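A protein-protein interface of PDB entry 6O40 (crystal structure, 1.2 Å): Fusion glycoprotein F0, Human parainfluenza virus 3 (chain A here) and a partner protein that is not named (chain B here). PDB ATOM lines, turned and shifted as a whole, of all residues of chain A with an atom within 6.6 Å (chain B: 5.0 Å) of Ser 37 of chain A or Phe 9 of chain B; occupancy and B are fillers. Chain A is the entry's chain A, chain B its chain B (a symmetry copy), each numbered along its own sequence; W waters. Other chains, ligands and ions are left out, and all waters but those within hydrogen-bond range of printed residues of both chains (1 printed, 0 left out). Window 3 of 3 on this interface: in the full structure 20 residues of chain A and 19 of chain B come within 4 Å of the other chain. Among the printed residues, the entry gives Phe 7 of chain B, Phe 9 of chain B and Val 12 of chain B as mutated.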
ATOM      1  N   ILE A  32      25.017  -7.568  -3.779  1.00  0.00           N
ATOM      2  CA  ILE A  32      23.981  -7.130  -2.835  1.00  0.00           C
ATOM      3  C   ILE A  32      23.432  -5.762  -3.248  1.00  0.00           C
ATOM      4  O   ILE A  32      22.217  -5.532  -3.253  1.00  0.00           O
ATOM      5  CB  ILE A  32      24.529  -7.093  -1.396  1.00  0.00           C
ATOM      6  CG1 ILE A  32      24.899  -8.496  -0.884  1.00  0.00           C
ATOM      7  CG2 ILE A  32      23.526  -6.424  -0.445  1.00  0.00           C
ATOM      8  CD1 ILE A  32      25.718  -8.506   0.424  1.00  0.00           C
ATOM      9  N   VAL A  33      24.331  -4.820  -3.533  1.00  0.00           N
ATOM     10  CA  VAL A  33      23.902  -3.492  -3.984  1.00  0.00           C
ATOM     11  C   VAL A  33      22.994  -3.595  -5.204  1.00  0.00           C
ATOM     12  O   VAL A  33      21.939  -2.942  -5.274  1.00  0.00           O
ATOM     13  CB  VAL A  33      25.126  -2.604  -4.280  1.00  0.00           C
ATOM     14  CG1 VAL A  33      24.711  -1.282  -4.947  1.00  0.00           C
ATOM     15  CG2 VAL A  33      25.950  -2.365  -3.025  1.00  0.00           C
ATOM     16  N   ALA A  34      23.394  -4.395  -6.190  1.00  0.00           N
ATOM     17  CA  ALA A  34      22.643  -4.582  -7.453  1.00  0.00           C
ATOM     18  C   ALA A  34      21.253  -5.172  -7.168  1.00  0.00           C
ATOM     19  O   ALA A  34      20.266  -4.621  -7.663  1.00  0.00           O
ATOM     20  CB  ALA A  34      23.436  -5.442  -8.403  1.00  0.00           C
ATOM     21  N   ILE A  35      21.170  -6.250  -6.391  1.00  0.00           N
ATOM     22  CA  ILE A  35      19.874  -6.917  -6.071  1.00  0.00           C
ATOM     23  C   ILE A  35      19.002  -5.959  -5.250  1.00  0.00           C
ATOM     24  O   ILE A  35      17.806  -5.903  -5.523  1.00  0.00           O
ATOM     25  CB  ILE A  35      20.110  -8.265  -5.369  1.00  0.00           C
ATOM     26  CG1 ILE A  35      20.751  -9.263  -6.332  1.00  0.00           C
ATOM     27  CG2 ILE A  35      18.817  -8.802  -4.778  1.00  0.00           C
ATOM     28  CD1 ILE A  35      21.287 -10.499  -5.666  1.00  0.00           C
ATOM     29  N   LYS A  36      19.582  -5.234  -4.296  1.00  0.00           N
ATOM     30  CA  LYS A  36      18.841  -4.251  -3.465  1.00  0.00           C
ATOM     31  C   LYS A  36      18.240  -3.193  -4.401  1.00  0.00           C
ATOM     32  O   LYS A  36      17.088  -2.807  -4.192  1.00  0.00           O
ATOM     33  CB  LYS A  36      19.756  -3.620  -2.415  1.00  0.00           C
ATOM     34  CG  LYS A  36      19.064  -2.648  -1.471  1.00  0.00           C
ATOM     35  CD  LYS A  36      20.000  -1.669  -0.797  1.00  0.00           C
ATOM     36  CE  LYS A  36      19.266  -0.671   0.075  1.00  0.00           C
ATOM     37  NZ  LYS A  36      19.540   0.727  -0.327  1.00  0.00           N
ATOM     38  N   SER A  37      19.000  -2.744  -5.398  1.00  0.00           N
ATOM     39  CA  SER A  37      18.541  -1.747  -6.397  1.00  0.00           C
ATOM     40  C   SER A  37      17.276  -2.272  -7.079  1.00  0.00           C
ATOM     41  O   SER A  37      16.293  -1.537  -7.157  1.00  0.00           O
ATOM     42  CB  SER A  37      19.613  -1.430  -7.396  1.00  0.00           C
ATOM     43  OG  SER A  37      19.244  -0.310  -8.181  1.00  0.00           O
ATOM     44  N   VAL A  38      17.311  -3.508  -7.565  1.00  0.00           N
ATOM     45  CA  VAL A  38      16.150  -4.149  -8.247  1.00  0.00           C
ATOM     46  C   VAL A  38      14.978  -4.213  -7.259  1.00  0.00           C
ATOM     47  O   VAL A  38      13.860  -3.903  -7.670  1.00  0.00           O
ATOM     48  CB  VAL A  38      16.513  -5.543  -8.783  1.00  0.00           C
ATOM     49  CG1 VAL A  38      15.300  -6.239  -9.371  1.00  0.00           C
ATOM     50  CG2 VAL A  38      17.644  -5.481  -9.793  1.00  0.00           C
ATOM     51  N   GLN A  39      15.244  -4.576  -6.003  1.00  0.00           N
ATOM     52  CA  GLN A  39      14.234  -4.683  -4.915  1.00  0.00           C
ATOM     53  C   GLN A  39      13.553  -3.325  -4.732  1.00  0.00           C
ATOM     54  O   GLN A  39      12.317  -3.268  -4.770  1.00  0.00           O
ATOM     55  CB  GLN A  39      14.892  -5.107  -3.598  1.00  0.00           C
ATOM     56  CG  GLN A  39      13.976  -5.015  -2.381  1.00  0.00           C
ATOM     57  CD  GLN A  39      14.747  -4.944  -1.084  1.00  0.00           C
ATOM     58  OE1 GLN A  39      15.854  -4.415  -1.023  1.00  0.00           O
ATOM     59  NE2 GLN A  39      14.167  -5.469  -0.020  1.00  0.00           N
ATOM     60  N   ASP A  40      14.352  -2.283  -4.530  1.00  0.00           N
ATOM     61  CA  ASP A  40      13.869  -0.900  -4.299  1.00  0.00           C
ATOM     62  C   ASP A  40      12.997  -0.478  -5.485  1.00  0.00           C
ATOM     63  O   ASP A  40      11.925   0.095  -5.242  1.00  0.00           O
ATOM     64  CB  ASP A  40      15.043   0.043  -4.034  1.00  0.00           C
ATOM     65  CG  ASP A  40      15.713  -0.198  -2.693  1.00  0.00           C
ATOM     66  OD1 ASP A  40      15.090  -0.838  -1.842  1.00  0.00           O
ATOM     67  OD2 ASP A  40      16.846   0.260  -2.515  1.00  0.00           O
ATOM     68  N   TYR A  41      13.413  -0.764  -6.719  1.00  0.00           N
ATOM     69  CA  TYR A  41      12.643  -0.373  -7.898  1.00  0.00           C
ATOM     70  C   TYR A  41      11.292  -1.081  -7.929  1.00  0.00           C
ATOM     71  O   TYR A  41      10.242  -0.455  -8.146  1.00  0.00           O
ATOM     72  CB  TYR A  41      13.448  -0.692  -9.163  1.00  0.00           C
ATOM     73  CG  TYR A  41      12.800  -0.203 -10.435  1.00  0.00           C
ATOM     74  CD1 TYR A  41      12.942   1.117 -10.843  1.00  0.00           C
ATOM     75  CD2 TYR A  41      12.034  -1.049 -11.223  1.00  0.00           C
ATOM     76  CE1 TYR A  41      12.344   1.573 -11.996  1.00  0.00           C
ATOM     77  CE2 TYR A  41      11.436  -0.597 -12.382  1.00  0.00           C
ATOM     78  CZ  TYR A  41      11.598   0.715 -12.761  1.00  0.00           C
ATOM     79  OH  TYR A  41      11.004   1.181 -13.915  1.00  0.00           O
ATOM     80  N   VAL A  42      11.293  -2.396  -7.716  1.00  0.00           N
ATOM     81  CA  VAL A  42      10.035  -3.135  -7.627  1.00  0.00           C
ATOM     82  C   VAL A  42       9.151  -2.562  -6.522  1.00  0.00           C
ATOM     83  O   VAL A  42       7.973  -2.244  -6.744  1.00  0.00           O
ATOM     84  CB  VAL A  42      10.308  -4.637  -7.421  1.00  0.00           C
ATOM     85  CG1 VAL A  42       9.020  -5.366  -7.028  1.00  0.00           C
ATOM     86  CG2 VAL A  42      10.926  -5.240  -8.683  1.00  0.00           C
ATOM     87  N   ALA B   3      16.556   3.290  -5.706  1.00  0.00           N
ATOM     88  CA  ALA B   3      17.077   2.407  -6.771  1.00  0.00           C
ATOM     89  C   ALA B   3      18.141   3.163  -7.567  1.00  0.00           C
ATOM     90  O   ALA B   3      17.964   4.366  -7.807  1.00  0.00           O
ATOM     91  CB  ALA B   3      15.955   1.964  -7.669  1.00  0.00           C
ATOM     92  N   LEU B   4      19.217   2.483  -7.954  1.00  0.00           N
ATOM     93  CA  LEU B   4      20.287   3.084  -8.783  1.00  0.00           C
ATOM     94  C   LEU B   4      19.715   3.401 -10.165  1.00  0.00           C
ATOM     95  O   LEU B   4      18.865   2.645 -10.634  1.00  0.00           O
ATOM     96  CB  LEU B   4      21.423   2.071  -8.932  1.00  0.00           C
ATOM     97  CG  LEU B   4      22.218   1.759  -7.671  1.00  0.00           C
ATOM     98  CD1 LEU B   4      23.214   0.650  -7.943  1.00  0.00           C
ATOM     99  CD2 LEU B   4      22.931   2.993  -7.166  1.00  0.00           C
ATOM    100  N   ASP B   5      20.147   4.496 -10.787  1.00  0.00           N
ATOM    101  CA  ASP B   5      19.758   4.763 -12.160  1.00  0.00           C
ATOM    102  C   ASP B   5      20.486   3.777 -13.080  1.00  0.00           C
ATOM    103  O   ASP B   5      21.385   3.050 -12.651  1.00  0.00           O
ATOM    104  CB  ASP B   5      19.924   6.248 -12.511  1.00  0.00           C
ATOM    105  CG  ASP B   5      21.352   6.678 -12.787  1.00  0.00           C
ATOM    106  OD1 ASP B   5      22.327   5.916 -12.610  1.00  0.00           O
ATOM    107  OD2 ASP B   5      21.538   7.850 -13.196  1.00  0.00           O
ATOM    108  N   PRO B   6      20.070   3.673 -14.333  1.00  0.00           N
ATOM    109  CA  PRO B   6      20.646   2.632 -15.196  1.00  0.00           C
ATOM    110  C   PRO B   6      22.142   2.777 -15.412  1.00  0.00           C
ATOM    111  O   PRO B   6      22.847   1.758 -15.482  1.00  0.00           O
ATOM    112  CB  PRO B   6      19.850   2.791 -16.502  1.00  0.00           C
ATOM    113  CG  PRO B   6      18.538   3.401 -16.066  1.00  0.00           C
ATOM    114  CD  PRO B   6      18.894   4.333 -14.944  1.00  0.00           C
ATOM    115  N   PHE B   7      22.655   4.010 -15.458  1.00  0.00           N
ATOM    116  CA  PHE B   7      24.087   4.226 -15.602  1.00  0.00           C
ATOM    117  C   PHE B   7      24.830   3.675 -14.397  1.00  0.00           C
ATOM    118  O   PHE B   7      25.793   2.923 -14.533  1.00  0.00           O
ATOM    119  CB  PHE B   7      24.365   5.731 -15.732  1.00  0.00           C
ATOM    120  CG  PHE B   7      25.788   6.063 -16.053  1.00  0.00           C
ATOM    121  CD1 PHE B   7      26.215   6.175 -17.367  1.00  0.00           C
ATOM    122  CD2 PHE B   7      26.704   6.284 -15.045  1.00  0.00           C
ATOM    123  CE1 PHE B   7      27.538   6.496 -17.648  1.00  0.00           C
ATOM    124  CE2 PHE B   7      28.019   6.598 -15.326  1.00  0.00           C
ATOM    125  CZ  PHE B   7      28.432   6.695 -16.625  1.00  0.00           C
ATOM    126  N   ASP B   8      24.411   4.065 -13.198  1.00  0.00           N
ATOM    127  CA  ASP B   8      25.073   3.639 -11.938  1.00  0.00           C
ATOM    128  C   ASP B   8      24.974   2.117 -11.796  1.00  0.00           C
ATOM    129  O   ASP B   8      25.926   1.521 -11.318  1.00  0.00           O
ATOM    130  CB  ASP B   8      24.497   4.377 -10.732  1.00  0.00           C
ATOM    131  CG  ASP B   8      25.036   5.787 -10.584  1.00  0.00           C
ATOM    132  OD1 ASP B   8      25.991   6.129 -11.288  1.00  0.00           O
ATOM    133  OD2 ASP B   8      24.495   6.520  -9.764  1.00  0.00           O
ATOM    134  N   PHE B   9      23.856   1.521 -12.199  1.00  0.00           N
ATOM    135  CA  PHE B   9      23.652   0.052 -12.147  1.00  0.00           C
ATOM    136  C   PHE B   9      24.717  -0.618 -13.025  1.00  0.00           C
ATOM    137  O   PHE B   9      25.313  -1.604 -12.597  1.00  0.00           O
ATOM    138  CB  PHE B   9      22.232  -0.322 -12.567  1.00  0.00           C
ATOM    139  CG  PHE B   9      21.869  -1.746 -12.241  1.00  0.00           C
ATOM    140  CD1 PHE B   9      21.284  -2.064 -11.031  1.00  0.00           C
ATOM    141  CD2 PHE B   9      22.143  -2.769 -13.130  1.00  0.00           C
ATOM    142  CE1 PHE B   9      20.954  -3.375 -10.729  1.00  0.00           C
ATOM    143  CE2 PHE B   9      21.816  -4.079 -12.821  1.00  0.00           C
ATOM    144  CZ  PHE B   9      21.225  -4.377 -11.620  1.00  0.00           C
ATOM    145  N   SER B  10      24.965  -0.067 -14.213  1.00  0.00           N
ATOM    146  CA  SER B  10      25.988  -0.566 -15.168  1.00  0.00           C
ATOM    147  C   SER B  10      27.374  -0.469 -14.521  1.00  0.00           C
ATOM    148  O   SER B  10      28.166  -1.392 -14.685  1.00  0.00           O
ATOM    149  CB  SER B  10      25.943   0.193 -16.466  1.00  0.00           C
ATOM    150  OG  SER B  10      24.846  -0.228 -17.256  1.00  0.00           O
ATOM    151  N   ILE B  11      27.659   0.628 -13.822  1.00  0.00           N
ATOM    152  CA  ILE B  11      28.967   0.818 -13.132  1.00  0.00           C
ATOM    153  C   ILE B  11      29.141  -0.313 -12.114  1.00  0.00           C
ATOM    154  O   ILE B  11      30.215  -0.908 -12.080  1.00  0.00           O
ATOM    155  CB  ILE B  11      29.059   2.200 -12.466  1.00  0.00           C
ATOM    156  CG1 ILE B  11      29.131   3.323 -13.503  1.00  0.00           C
ATOM    157  CG2 ILE B  11      30.240   2.244 -11.514  1.00  0.00           C
ATOM    158  CD1 ILE B  11      30.345   3.243 -14.388  1.00  0.00           C
ATOM    159  N   VAL B  12      28.107  -0.598 -11.327  1.00  0.00           N
ATOM    160  CA  VAL B  12      28.145  -1.662 -10.279  1.00  0.00           C
ATOM    161  C   VAL B  12      28.378  -3.022 -10.945  1.00  0.00           C
ATOM    162  O   VAL B  12      29.242  -3.758 -10.469  1.00  0.00           O
ATOM    163  CB  VAL B  12      26.873  -1.655  -9.412  1.00  0.00           C
ATOM    164  CG1 VAL B  12      26.819  -2.852  -8.474  1.00  0.00           C
ATOM    165  CG2 VAL B  12      26.749  -0.356  -8.634  1.00  0.00           C
ATOM    166  N   LEU B  13      27.655  -3.352 -12.014  1.00  0.00           N
ATOM    167  CA  LEU B  13      27.823  -4.665 -12.688  1.00  0.00           C
ATOM    168  C   LEU B  13      29.255  -4.794 -13.207  1.00  0.00           C
ATOM    169  O   LEU B  13      29.822  -5.873 -13.094  1.00  0.00           O
ATOM    170  CB  LEU B  13      26.830  -4.794 -13.842  1.00  0.00           C
ATOM    171  CG  LEU B  13      25.372  -4.962 -13.435  1.00  0.00           C
ATOM    172  CD1 LEU B  13      24.571  -5.550 -14.587  1.00  0.00           C
ATOM    173  CD2 LEU B  13      25.249  -5.820 -12.185  1.00  0.00           C
HETATM  174  O   HOH W   1      18.037  -0.012 -10.664  1.00  0.00           O
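Printed residues of chain B that touch a printed residue of chain A: Ala 3, Leu 4 and Phe 9.
Hydrophobic or aromatic side chains of chain B within 4 Å of the printed part of chain A: Ala 3, Leu 4 and Phe 9.
Along chain B the printed residues that touch a printed residue of chain A span positions 3 to 9.
Of the 11 printed residues of chain A, 5 touch a printed residue of chain B.
Printed residues of chain A that touch a printed residue of chain B: Val 33, Ala 34, Ser 37, Asp 40 and Tyr 41.
Hydrophobic or aromatic side chains of chain A within 4 Å of the printed part of chain B: Val 33, Ala 34 and Tyr 41.
Among the printed residues, no Asp or Glu carboxylate lies within 4 Å of a Lys or Arg side-chain nitrogen of the other chain.
Ser 37 of chain A touches three residues of chain B.
Of chain A, only Ala 34 and Ser 37 come within 4 Å of Phe 9 of chain B.
Printed residues of chain A within 4 Å of Leu 4 of chain B: Val 33 (3.9 Å) and Ser 37 (2.8 Å).
Printed residues of chain A within 4 Å of Ala 3 of chain B: Ser 37, Asp 40 and Tyr 41.
Of the printed residues of chain B, Ala 34 of chain A touches Phe 9.
Of the printed residues of chain B, Val 33 of chain A touches Leu 4.
Printed residues of chain B within 4 Å of Asp 40 of chain A: Ala 3.
Val 38 of chain A touches none of the printed residues of chain B.
The nearest printed residue of chain B that does not touch Tyr 41 of chain A is Leu 4 of chain B (6.1 Å).
The side-chain hydroxyl of Ser 37 of chain A lies within hydrogen-bond range of the backbone NH of Leu 4 of chain B, at 2.8 Å.
Water W1 bridges OG of Ser 37 of chain A (2.8 Å) and O of Leu 4 of chain B (2.8 Å).
The side-chain amino group (NZ) of Lys 36 of chain A lies within salt-bridge range of the side-chain carboxylate (OD2) of Asp 40 of chain A, 3.5 Å away.
Among the printed residues, merely in contact across the chains: Ala 34 of chain A with Phe 9 of chain B, Ser 37 of chain A with Ala 3 of chain B, Tyr 41 of chain A with Ala 3 of chain B, Val 33 of chain A with Leu 4 of chain B, Ser 37 of chain A with Phe 9 of chain B and Asp 40 of chain A with Ala 3 of chain B.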
